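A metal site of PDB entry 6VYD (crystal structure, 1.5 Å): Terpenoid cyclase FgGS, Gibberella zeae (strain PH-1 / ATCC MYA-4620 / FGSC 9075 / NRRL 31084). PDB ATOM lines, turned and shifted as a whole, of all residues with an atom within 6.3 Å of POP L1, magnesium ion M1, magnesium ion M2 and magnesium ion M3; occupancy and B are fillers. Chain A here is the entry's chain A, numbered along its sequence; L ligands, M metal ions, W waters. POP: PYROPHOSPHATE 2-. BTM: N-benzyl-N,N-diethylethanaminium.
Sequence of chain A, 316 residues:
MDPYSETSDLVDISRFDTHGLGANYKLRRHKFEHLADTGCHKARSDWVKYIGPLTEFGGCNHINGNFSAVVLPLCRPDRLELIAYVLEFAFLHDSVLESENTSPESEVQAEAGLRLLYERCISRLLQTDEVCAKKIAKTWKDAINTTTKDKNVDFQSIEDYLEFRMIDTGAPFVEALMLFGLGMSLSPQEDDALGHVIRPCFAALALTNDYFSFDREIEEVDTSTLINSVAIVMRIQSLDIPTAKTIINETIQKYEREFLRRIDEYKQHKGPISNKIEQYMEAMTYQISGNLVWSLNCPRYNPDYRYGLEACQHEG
Magnesium ion M3 is bound by water W2, water W3, the side-chain carboxylate (OD1) of Asp 94, the side-chain carboxylate (OE2) of Glu 98, water W1 and an oxygen (O2) of POP L1. Magnesium ion M3 has six donor atoms within binding distance.
Magnesium ion M2 is bound by O2 of POP L1, O5 of POP L1, water W7, OD2 of Asp 94, OE2 of Glu 98 and water W5. Magnesium ion M2 has six donor atoms within binding distance.
Hydrophobic or aromatic side chains that line POP L1: Tyr 301. Within 4 Å of POP L1: Asp 94, Glu 98, Arg 165, Thr 169, Asn 209, Ser 213, Arg 216, Glu 217, Arg 300 and Tyr 301. Along chain A the residues within 4 Å of POP L1 span positions 94 to 301. The nearest printed residue that does not touch POP L1 is Phe 91 (4.02 Å).
OD1 of Asp 168 touches magnesium ion M3 (3.98 Å). Of the 21 residues printed, 3 come within 4 Å of magnesium ion M3.
Merely in contact with magnesium ion M1: Arg 165 (3.8 Å). Along chain A the residues within 4 Å of magnesium ion M1 span positions 165 to 217. The nearest printed residue that does not touch magnesium ion M1 is Arg 216 (4.5 Å).
The side-chain carboxylate of Glu 217 sits close to the guanidinium group of Arg 216. ND2 of Asn 228 lies within hydrogen-bond range of OE2 of Glu 217 (2.9 Å). The side-chain amide nitrogen of Asn 209 is in hydrogen-bond range of the side-chain hydroxyl of Tyr 301 (2.7 Å). The side-chain amide oxygen (OD1) of Asn 209 lies close to the guanidinium group (NH2) of Arg 165 (3.0 Å). The guanidinium group of Arg 300 is in hydrogen-bond range of the backbone carbonyl oxygen of Phe 91 (3.1 Å). The guanidinium group (NH2) of Arg 300 lies within hydrogen-bond range of the side-chain hydroxyl (OG) of Ser 95 (3.3 Å). NH2 of Arg 165 is in salt-bridge range of OD2 of Asp 210 (2.9 Å). The side-chain carboxylate of Asp 168 lies within hydrogen-bond range of the side-chain hydroxyl of Thr 147, 2.6 Å away.
Magnesium ion M1 is bound by an oxygen (O1) of POP L1 (2.0 Å), an oxygen (O6) of POP L1 (2.1 Å), the side-chain carboxylate of Glu 217 (2.1 Å), the side-chain amide oxygen of Asn 209 (2.1 Å), water W4 (2.1 Å) and the side-chain hydroxyl of Ser 213 (2.3 Å).
Residues that only touch magnesium ion M2: Arg 216 and Arg 300. Within 4 Å of magnesium ion M2: Asp 94, Glu 98, Arg 216 and Arg 300. Along chain A the residues within 4 Å of magnesium ion M2 span positions 94 to 300. The nearest printed residue that does not touch magnesium ion M2 is Glu 217 (4.4 Å).
Water W7 bridges OE1 of Glu 98 and NH1 of Arg 216. Water W5 lies within hydrogen-bond range of the side-chain hydroxyl of Ser 95 (2.7 Å), the guanidinium group of Arg 216 (3.1 Å) and the guanidinium group of Arg 300 (3.4 Å). Water W3 lies within hydrogen-bond range of O3 of POP L1 (2.7 Å) and O of Asp 168 (2.7 Å). Water W2 bridges the side-chain carboxylate of Asp 168 (2.7 Å) and the guanidinium group of Arg 165 (3.4 Å).
OH of Tyr 301 is in hydrogen-bond range of O4 of POP L1 (2.5 Å). O4 of POP L1 lies within salt-bridge range of NE of Arg 300, at 2.8 Å. The guanidinium group (NH1) of Arg 165 is in salt-bridge range of an oxygen (O3) of POP L1, at 2.8 Å. The guanidinium group (NH1) of Arg 216 lies close to an oxygen (O5) of POP L1 (2.8 Å). The side-chain hydroxyl of Thr 169 is in hydrogen-bond range of an oxygen (O3) of POP L1, at 2.9 Å.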
ATOM      1  N   PHE A  91     -11.121   9.515 -20.702  1.00  0.00           N
ATOM      2  CA  PHE A  91     -10.961  10.030 -22.063  1.00  0.00           C
ATOM      3  C   PHE A  91     -11.741  11.333 -22.245  1.00  0.00           C
ATOM      4  O   PHE A  91     -11.268  12.265 -22.916  1.00  0.00           O
ATOM      5  CB  PHE A  91     -11.525   9.015 -23.060  1.00  0.00           C
ATOM      6  CG  PHE A  91     -10.527   8.022 -23.587  1.00  0.00           C
ATOM      7  CD1 PHE A  91      -9.511   8.392 -24.455  1.00  0.00           C
ATOM      8  CD2 PHE A  91     -10.677   6.663 -23.277  1.00  0.00           C
ATOM      9  CE1 PHE A  91      -8.639   7.443 -24.975  1.00  0.00           C
ATOM     10  CE2 PHE A  91      -9.802   5.724 -23.765  1.00  0.00           C
ATOM     11  CZ  PHE A  91      -8.785   6.084 -24.613  1.00  0.00           C
ATOM     12  N   ASP A  94     -10.373  14.182 -20.023  1.00  0.00           N
ATOM     13  CA  ASP A  94      -9.104  14.644 -20.583  1.00  0.00           C
ATOM     14  C   ASP A  94      -9.320  15.847 -21.503  1.00  0.00           C
ATOM     15  O   ASP A  94      -8.611  16.869 -21.418  1.00  0.00           O
ATOM     16  CB  ASP A  94      -8.486  13.463 -21.361  1.00  0.00           C
ATOM     17  CG  ASP A  94      -7.345  13.903 -22.254  1.00  0.00           C
ATOM     18  OD1 ASP A  94      -6.290  14.318 -21.703  1.00  0.00           O
ATOM     19  OD2 ASP A  94      -7.526  13.896 -23.493  1.00  0.00           O
ATOM     20  N   SER A  95     -10.291  15.745 -22.408  1.00  0.00           N
ATOM     21  CA  SER A  95     -10.506  16.853 -23.335  1.00  0.00           C
ATOM     22  C   SER A  95     -11.009  18.104 -22.617  1.00  0.00           C
ATOM     23  O   SER A  95     -10.701  19.226 -23.031  1.00  0.00           O
ATOM     24  CB  SER A  95     -11.440  16.382 -24.467  1.00  0.00           C
ATOM     25  OG  SER A  95     -10.853  15.262 -25.106  1.00  0.00           O
ATOM     26  N   GLU A  98      -7.923  19.844 -21.254  1.00  0.00           N
ATOM     27  CA  GLU A  98      -7.129  20.515 -22.271  1.00  0.00           C
ATOM     28  C   GLU A  98      -7.868  21.689 -22.899  1.00  0.00           C
ATOM     29  O   GLU A  98      -7.236  22.534 -23.559  1.00  0.00           O
ATOM     30  CB  GLU A  98      -6.751  19.516 -23.378  1.00  0.00           C
ATOM     31  CG  GLU A  98      -5.790  18.377 -22.997  1.00  0.00           C
ATOM     32  CD  GLU A  98      -5.586  17.406 -24.149  1.00  0.00           C
ATOM     33  OE1 GLU A  98      -5.383  17.874 -25.308  1.00  0.00           O
ATOM     34  OE2 GLU A  98      -5.640  16.182 -23.903  1.00  0.00           O
ATOM     35  N   THR A 147      -1.691  17.903 -15.268  1.00  0.00           N
ATOM     36  CA  THR A 147      -2.230  18.554 -16.469  1.00  0.00           C
ATOM     37  C   THR A 147      -2.678  19.975 -16.168  1.00  0.00           C
ATOM     38  O   THR A 147      -2.330  20.919 -16.892  1.00  0.00           O
ATOM     39  CB  THR A 147      -3.418  17.742 -16.995  1.00  0.00           C
ATOM     40  OG1 THR A 147      -2.943  16.437 -17.371  1.00  0.00           O
ATOM     41  CG2 THR A 147      -4.003  18.449 -18.203  1.00  0.00           C
ATOM     42  N   ARG A 165       4.818  14.603 -19.745  1.00  0.00           N
ATOM     43  CA  ARG A 165       3.836  13.930 -20.602  1.00  0.00           C
ATOM     44  C   ARG A 165       3.482  12.534 -20.093  1.00  0.00           C
ATOM     45  O   ARG A 165       2.333  12.102 -20.272  1.00  0.00           O
ATOM     46  CB  ARG A 165       4.394  13.841 -22.019  1.00  0.00           C
ATOM     47  CG  ARG A 165       3.373  13.380 -23.078  1.00  0.00           C
ATOM     48  CD  ARG A 165       2.185  14.336 -23.274  1.00  0.00           C
ATOM     49  NE  ARG A 165       1.472  13.784 -24.421  1.00  0.00           N
ATOM     50  CZ  ARG A 165       0.270  13.245 -24.368  1.00  0.00           C
ATOM     51  NH1 ARG A 165      -0.503  13.383 -23.265  1.00  0.00           N
ATOM     52  NH2 ARG A 165      -0.142  12.535 -25.424  1.00  0.00           N
ATOM     53  N   ASP A 168       0.811  13.398 -17.662  1.00  0.00           N
ATOM     54  CA  ASP A 168      -0.331  14.021 -18.325  1.00  0.00           C
ATOM     55  C   ASP A 168      -1.142  12.988 -19.109  1.00  0.00           C
ATOM     56  O   ASP A 168      -2.389  13.040 -19.125  1.00  0.00           O
ATOM     57  CB  ASP A 168       0.184  15.118 -19.271  1.00  0.00           C
ATOM     58  CG  ASP A 168      -0.886  15.680 -20.230  1.00  0.00           C
ATOM     59  OD1 ASP A 168      -0.716  15.533 -21.458  1.00  0.00           O
ATOM     60  OD2 ASP A 168      -1.823  16.333 -19.751  1.00  0.00           O
ATOM     61  N   THR A 169      -0.464  12.049 -19.785  1.00  0.00           N
ATOM     62  CA  THR A 169      -1.211  11.037 -20.542  1.00  0.00           C
ATOM     63  C   THR A 169      -1.792   9.968 -19.626  1.00  0.00           C
ATOM     64  O   THR A 169      -2.579   9.132 -20.073  1.00  0.00           O
ATOM     65  CB  THR A 169      -0.326  10.452 -21.670  1.00  0.00           C
ATOM     66  OG1 THR A 169      -1.133   9.921 -22.747  1.00  0.00           O
ATOM     67  CG2 THR A 169       0.609   9.354 -21.140  1.00  0.00           C
ATOM     68  N   GLY A 170      -1.441   9.989 -18.340  1.00  0.00           N
ATOM     69  CA  GLY A 170      -1.993   9.007 -17.417  1.00  0.00           C
ATOM     70  C   GLY A 170      -1.370   7.635 -17.522  1.00  0.00           C
ATOM     71  O   GLY A 170      -2.050   6.625 -17.247  1.00  0.00           O
ATOM     72  N   ALA A 206       3.295   7.396 -24.718  1.00  0.00           N
ATOM     73  CA  ALA A 206       2.914   8.810 -24.879  1.00  0.00           C
ATOM     74  C   ALA A 206       3.268   9.300 -26.273  1.00  0.00           C
ATOM     75  O   ALA A 206       2.452   9.961 -26.930  1.00  0.00           O
ATOM     76  CB  ALA A 206       3.657   9.653 -23.827  1.00  0.00           C
ATOM     77  N   ASN A 209       0.921   7.840 -28.851  1.00  0.00           N
ATOM     78  CA  ASN A 209      -0.282   8.644 -28.849  1.00  0.00           C
ATOM     79  C   ASN A 209      -0.080   9.943 -29.629  1.00  0.00           C
ATOM     80  O   ASN A 209      -0.925  10.323 -30.449  1.00  0.00           O
ATOM     81  CB  ASN A 209      -0.788   8.939 -27.448  1.00  0.00           C
ATOM     82  CG  ASN A 209      -1.970   9.859 -27.506  1.00  0.00           C
ATOM     83  OD1 ASN A 209      -1.798  11.087 -27.495  1.00  0.00           O
ATOM     84  ND2 ASN A 209      -3.179   9.289 -27.681  1.00  0.00           N
ATOM     85  N   ASP A 210       1.022  10.662 -29.351  1.00  0.00           N
ATOM     86  CA  ASP A 210       1.262  11.918 -30.061  1.00  0.00           C
ATOM     87  C   ASP A 210       1.257  11.702 -31.564  1.00  0.00           C
ATOM     88  O   ASP A 210       0.666  12.494 -32.306  1.00  0.00           O
ATOM     89  CB  ASP A 210       2.632  12.485 -29.661  1.00  0.00           C
ATOM     90  CG  ASP A 210       2.681  13.049 -28.257  1.00  0.00           C
ATOM     91  OD1 ASP A 210       3.795  13.356 -27.833  1.00  0.00           O
ATOM     92  OD2 ASP A 210       1.646  13.197 -27.599  1.00  0.00           O
ATOM     93  N   SER A 213      -2.441  10.906 -32.798  1.00  0.00           N
ATOM     94  CA  SER A 213      -3.465  11.887 -32.446  1.00  0.00           C
ATOM     95  C   SER A 213      -3.100  13.322 -32.866  1.00  0.00           C
ATOM     96  O   SER A 213      -3.932  14.215 -32.680  1.00  0.00           O
ATOM     97  CB  SER A 213      -3.782  11.840 -30.942  1.00  0.00           C
ATOM     98  OG  SER A 213      -2.662  12.219 -30.102  1.00  0.00           O
ATOM     99  N   PHE A 214      -1.920  13.534 -33.428  1.00  0.00           N
ATOM    100  CA  PHE A 214      -1.494  14.863 -33.871  1.00  0.00           C
ATOM    101  C   PHE A 214      -2.508  15.528 -34.796  1.00  0.00           C
ATOM    102  O   PHE A 214      -2.863  16.696 -34.604  1.00  0.00           O
ATOM    103  CB  PHE A 214      -0.125  14.793 -34.553  1.00  0.00           C
ATOM    104  CG  PHE A 214       0.336  16.091 -35.130  1.00  0.00           C
ATOM    105  CD1 PHE A 214       1.011  17.025 -34.347  1.00  0.00           C
ATOM    106  CD2 PHE A 214       0.101  16.392 -36.464  1.00  0.00           C
ATOM    107  CE1 PHE A 214       1.430  18.250 -34.879  1.00  0.00           C
ATOM    108  CE2 PHE A 214       0.502  17.611 -37.009  1.00  0.00           C
ATOM    109  CZ  PHE A 214       1.183  18.525 -36.216  1.00  0.00           C
ATOM    110  N   ARG A 216      -5.658  15.165 -35.306  1.00  0.00           N
ATOM    111  CA  ARG A 216      -6.867  15.540 -34.580  1.00  0.00           C
ATOM    112  C   ARG A 216      -6.584  16.696 -33.623  1.00  0.00           C
ATOM    113  O   ARG A 216      -7.430  17.588 -33.441  1.00  0.00           O
ATOM    114  CB  ARG A 216      -7.399  14.267 -33.871  1.00  0.00           C
ATOM    115  CG  ARG A 216      -8.459  14.488 -32.820  1.00  0.00           C
ATOM    116  CD  ARG A 216      -7.849  14.525 -31.459  1.00  0.00           C
ATOM    117  NE  ARG A 216      -8.825  14.410 -30.392  1.00  0.00           N
ATOM    118  CZ  ARG A 216      -8.487  14.118 -29.139  1.00  0.00           C
ATOM    119  NH1 ARG A 216      -7.191  13.975 -28.843  1.00  0.00           N
ATOM    120  NH2 ARG A 216      -9.409  14.023 -28.183  1.00  0.00           N
ATOM    121  N   GLU A 217      -5.416  16.680 -32.974  1.00  0.00           N
ATOM    122  CA  GLU A 217      -5.104  17.751 -32.021  1.00  0.00           C
ATOM    123  C   GLU A 217      -4.841  19.096 -32.707  1.00  0.00           C
ATOM    124  O   GLU A 217      -5.091  20.162 -32.117  1.00  0.00           O
ATOM    125  CB  GLU A 217      -3.997  17.322 -31.061  1.00  0.00           C
ATOM    126  CG  GLU A 217      -4.472  16.130 -30.212  1.00  0.00           C
ATOM    127  CD  GLU A 217      -3.403  15.475 -29.378  1.00  0.00           C
ATOM    128  OE1 GLU A 217      -3.785  14.535 -28.624  1.00  0.00           O
ATOM    129  OE2 GLU A 217      -2.204  15.901 -29.464  1.00  0.00           O
ATOM    130  N   ILE A 227      -0.604  19.608 -26.848  1.00  0.00           N
ATOM    131  CA  ILE A 227       0.411  18.890 -26.062  1.00  0.00           C
ATOM    132  C   ILE A 227       0.855  17.728 -26.947  1.00  0.00           C
ATOM    133  O   ILE A 227       0.202  16.674 -26.992  1.00  0.00           O
ATOM    134  CB  ILE A 227      -0.132  18.418 -24.712  1.00  0.00           C
ATOM    135  CG1 ILE A 227      -0.682  19.592 -23.890  1.00  0.00           C
ATOM    136  CG2 ILE A 227       0.879  17.568 -23.933  1.00  0.00           C
ATOM    137  CD1 ILE A 227      -1.601  19.200 -22.723  1.00  0.00           C
ATOM    138  N   ASN A 228       1.952  17.909 -27.690  1.00  0.00           N
ATOM    139  CA  ASN A 228       2.262  16.914 -28.693  1.00  0.00           C
ATOM    140  C   ASN A 228       3.704  17.068 -29.176  1.00  0.00           C
ATOM    141  O   ASN A 228       4.095  18.151 -29.669  1.00  0.00           O
ATOM    142  CB  ASN A 228       1.278  17.036 -29.877  1.00  0.00           C
ATOM    143  CG  ASN A 228       1.329  15.817 -30.809  1.00  0.00           C
ATOM    144  OD1 ASN A 228       2.408  15.474 -31.344  1.00  0.00           O
ATOM    145  ND2 ASN A 228       0.188  15.113 -30.942  1.00  0.00           N
ATOM    146  N   TRP A 294      -4.911   0.011 -31.570  1.00  0.00           N
ATOM    147  CA  TRP A 294      -6.136   0.786 -31.378  1.00  0.00           C
ATOM    148  C   TRP A 294      -6.038   2.153 -32.046  1.00  0.00           C
ATOM    149  O   TRP A 294      -7.007   2.621 -32.663  1.00  0.00           O
ATOM    150  CB  TRP A 294      -6.390   0.930 -29.873  1.00  0.00           C
ATOM    151  CG  TRP A 294      -7.496   1.879 -29.518  1.00  0.00           C
ATOM    152  CD1 TRP A 294      -8.838   1.612 -29.461  1.00  0.00           C
ATOM    153  CD2 TRP A 294      -7.340   3.265 -29.133  1.00  0.00           C
ATOM    154  NE1 TRP A 294      -9.533   2.745 -29.070  1.00  0.00           N
ATOM    155  CE2 TRP A 294      -8.639   3.774 -28.876  1.00  0.00           C
ATOM    156  CE3 TRP A 294      -6.242   4.123 -28.993  1.00  0.00           C
ATOM    157  CZ2 TRP A 294      -8.864   5.104 -28.466  1.00  0.00           C
ATOM    158  CZ3 TRP A 294      -6.457   5.438 -28.566  1.00  0.00           C
ATOM    159  CH2 TRP A 294      -7.754   5.917 -28.331  1.00  0.00           C
ATOM    160  N   ARG A 300     -11.742   8.187 -32.277  1.00  0.00           N
ATOM    161  CA  ARG A 300     -11.290   9.408 -31.594  1.00  0.00           C
ATOM    162  C   ARG A 300     -10.314  10.191 -32.446  1.00  0.00           C
ATOM    163  O   ARG A 300     -10.365  11.428 -32.467  1.00  0.00           O
ATOM    164  CB  ARG A 300     -10.669   9.022 -30.252  1.00  0.00           C
ATOM    165  CG  ARG A 300     -10.306  10.240 -29.343  1.00  0.00           C
ATOM    166  CD  ARG A 300      -9.850   9.681 -27.991  1.00  0.00           C
ATOM    167  NE  ARG A 300      -9.289  10.667 -27.067  1.00  0.00           N
ATOM    168  CZ  ARG A 300     -10.023  11.380 -26.217  1.00  0.00           C
ATOM    169  NH1 ARG A 300     -11.353  11.234 -26.216  1.00  0.00           N
ATOM    170  NH2 ARG A 300      -9.448  12.270 -25.400  1.00  0.00           N
ATOM    171  N   TYR A 301      -9.394   9.510 -33.151  1.00  0.00           N
ATOM    172  CA  TYR A 301      -8.358  10.228 -33.905  1.00  0.00           C
ATOM    173  C   TYR A 301      -8.591  10.240 -35.402  1.00  0.00           C
ATOM    174  O   TYR A 301      -7.934  11.002 -36.116  1.00  0.00           O
ATOM    175  CB  TYR A 301      -6.949   9.662 -33.702  1.00  0.00           C
ATOM    176  CG  TYR A 301      -6.605   9.444 -32.247  1.00  0.00           C
ATOM    177  CD1 TYR A 301      -7.123  10.279 -31.244  1.00  0.00           C
ATOM    178  CD2 TYR A 301      -5.804   8.360 -31.871  1.00  0.00           C
ATOM    179  CE1 TYR A 301      -6.827  10.035 -29.904  1.00  0.00           C
ATOM    180  CE2 TYR A 301      -5.508   8.116 -30.530  1.00  0.00           C
ATOM    181  CZ  TYR A 301      -6.044   8.931 -29.558  1.00  0.00           C
ATOM    182  OH  TYR A 301      -5.772   8.656 -28.249  1.00  0.00           O
HETATM  183  P1  POP L   1      -3.730  12.677 -24.758  1.00  0.00           P
HETATM  184  O1  POP L   1      -2.992  13.178 -25.965  1.00  0.00           O
HETATM  185  O2  POP L   1      -4.695  13.698 -24.201  1.00  0.00           O
HETATM  186  O3  POP L   1      -2.890  12.004 -23.723  1.00  0.00           O
HETATM  187  O   POP L   1      -4.752  11.505 -25.262  1.00  0.00           O
HETATM  188  P2  POP L   1      -5.706  11.707 -26.567  1.00  0.00           P
HETATM  189  O4  POP L   1      -6.564  10.462 -26.634  1.00  0.00           O
HETATM  190  O5  POP L   1      -6.533  12.925 -26.284  1.00  0.00           O
HETATM  191  O6  POP L   1      -4.834  11.879 -27.754  1.00  0.00           O
HETATM  192  N   BTM L   2      -4.756   7.728 -22.734  1.00  0.00           N
HETATM  193  C1  BTM L   2      -3.164   7.615 -22.874  1.00  0.00           C
HETATM  194  C2  BTM L   2      -5.254   7.059 -21.432  1.00  0.00           C
HETATM  195  C3  BTM L   2      -6.767   7.125 -21.231  1.00  0.00           C
HETATM  196  C4  BTM L   2      -5.035   9.314 -22.706  1.00  0.00           C
HETATM  197  C5  BTM L   2      -6.411   9.763 -23.106  1.00  0.00           C
HETATM  198  C6  BTM L   2      -5.490   6.987 -23.935  1.00  0.00           C
HETATM  199  C7  BTM L   2      -4.961   7.458 -25.289  1.00  0.00           C
HETATM  200  C8  BTM L   2      -2.606   6.262 -22.633  1.00  0.00           C
HETATM  201  C9  BTM L   2      -2.102   5.882 -21.384  1.00  0.00           C
HETATM  202  C10 BTM L   2      -1.576   4.596 -21.232  1.00  0.00           C
HETATM  203  C11 BTM L   2      -1.538   3.681 -22.269  1.00  0.00           C
HETATM  204  C12 BTM L   2      -1.961   4.085 -23.516  1.00  0.00           C
HETATM  205  C13 BTM L   2      -2.487   5.358 -23.685  1.00  0.00           C
HETATM  206 MG    MG M   1      -2.971  12.762 -27.928  1.00  0.00          MG
HETATM  207 MG    MG M   2      -6.309  14.545 -25.081  1.00  0.00          MG
HETATM  208 MG    MG M   3      -4.517  15.037 -22.541  1.00  0.00          MG
HETATM  209  O   HOH W   1      -4.330  16.286 -20.830  1.00  0.00           O
HETATM  210  O   HOH W   2      -2.814  15.914 -23.172  1.00  0.00           O
HETATM  211  O   HOH W   3      -3.595  13.465 -21.533  1.00  0.00           O
HETATM  212  O   HOH W   4      -1.084  13.726 -28.141  1.00  0.00           O
HETATM  213  O   HOH W   5      -8.194  15.466 -25.699  1.00  0.00           O
HETATM  214  O   HOH W   6      -2.155  15.793 -25.835  1.00  0.00           O
HETATM  215  O   HOH W   7      -5.441  15.558 -26.701  1.00  0.00           O
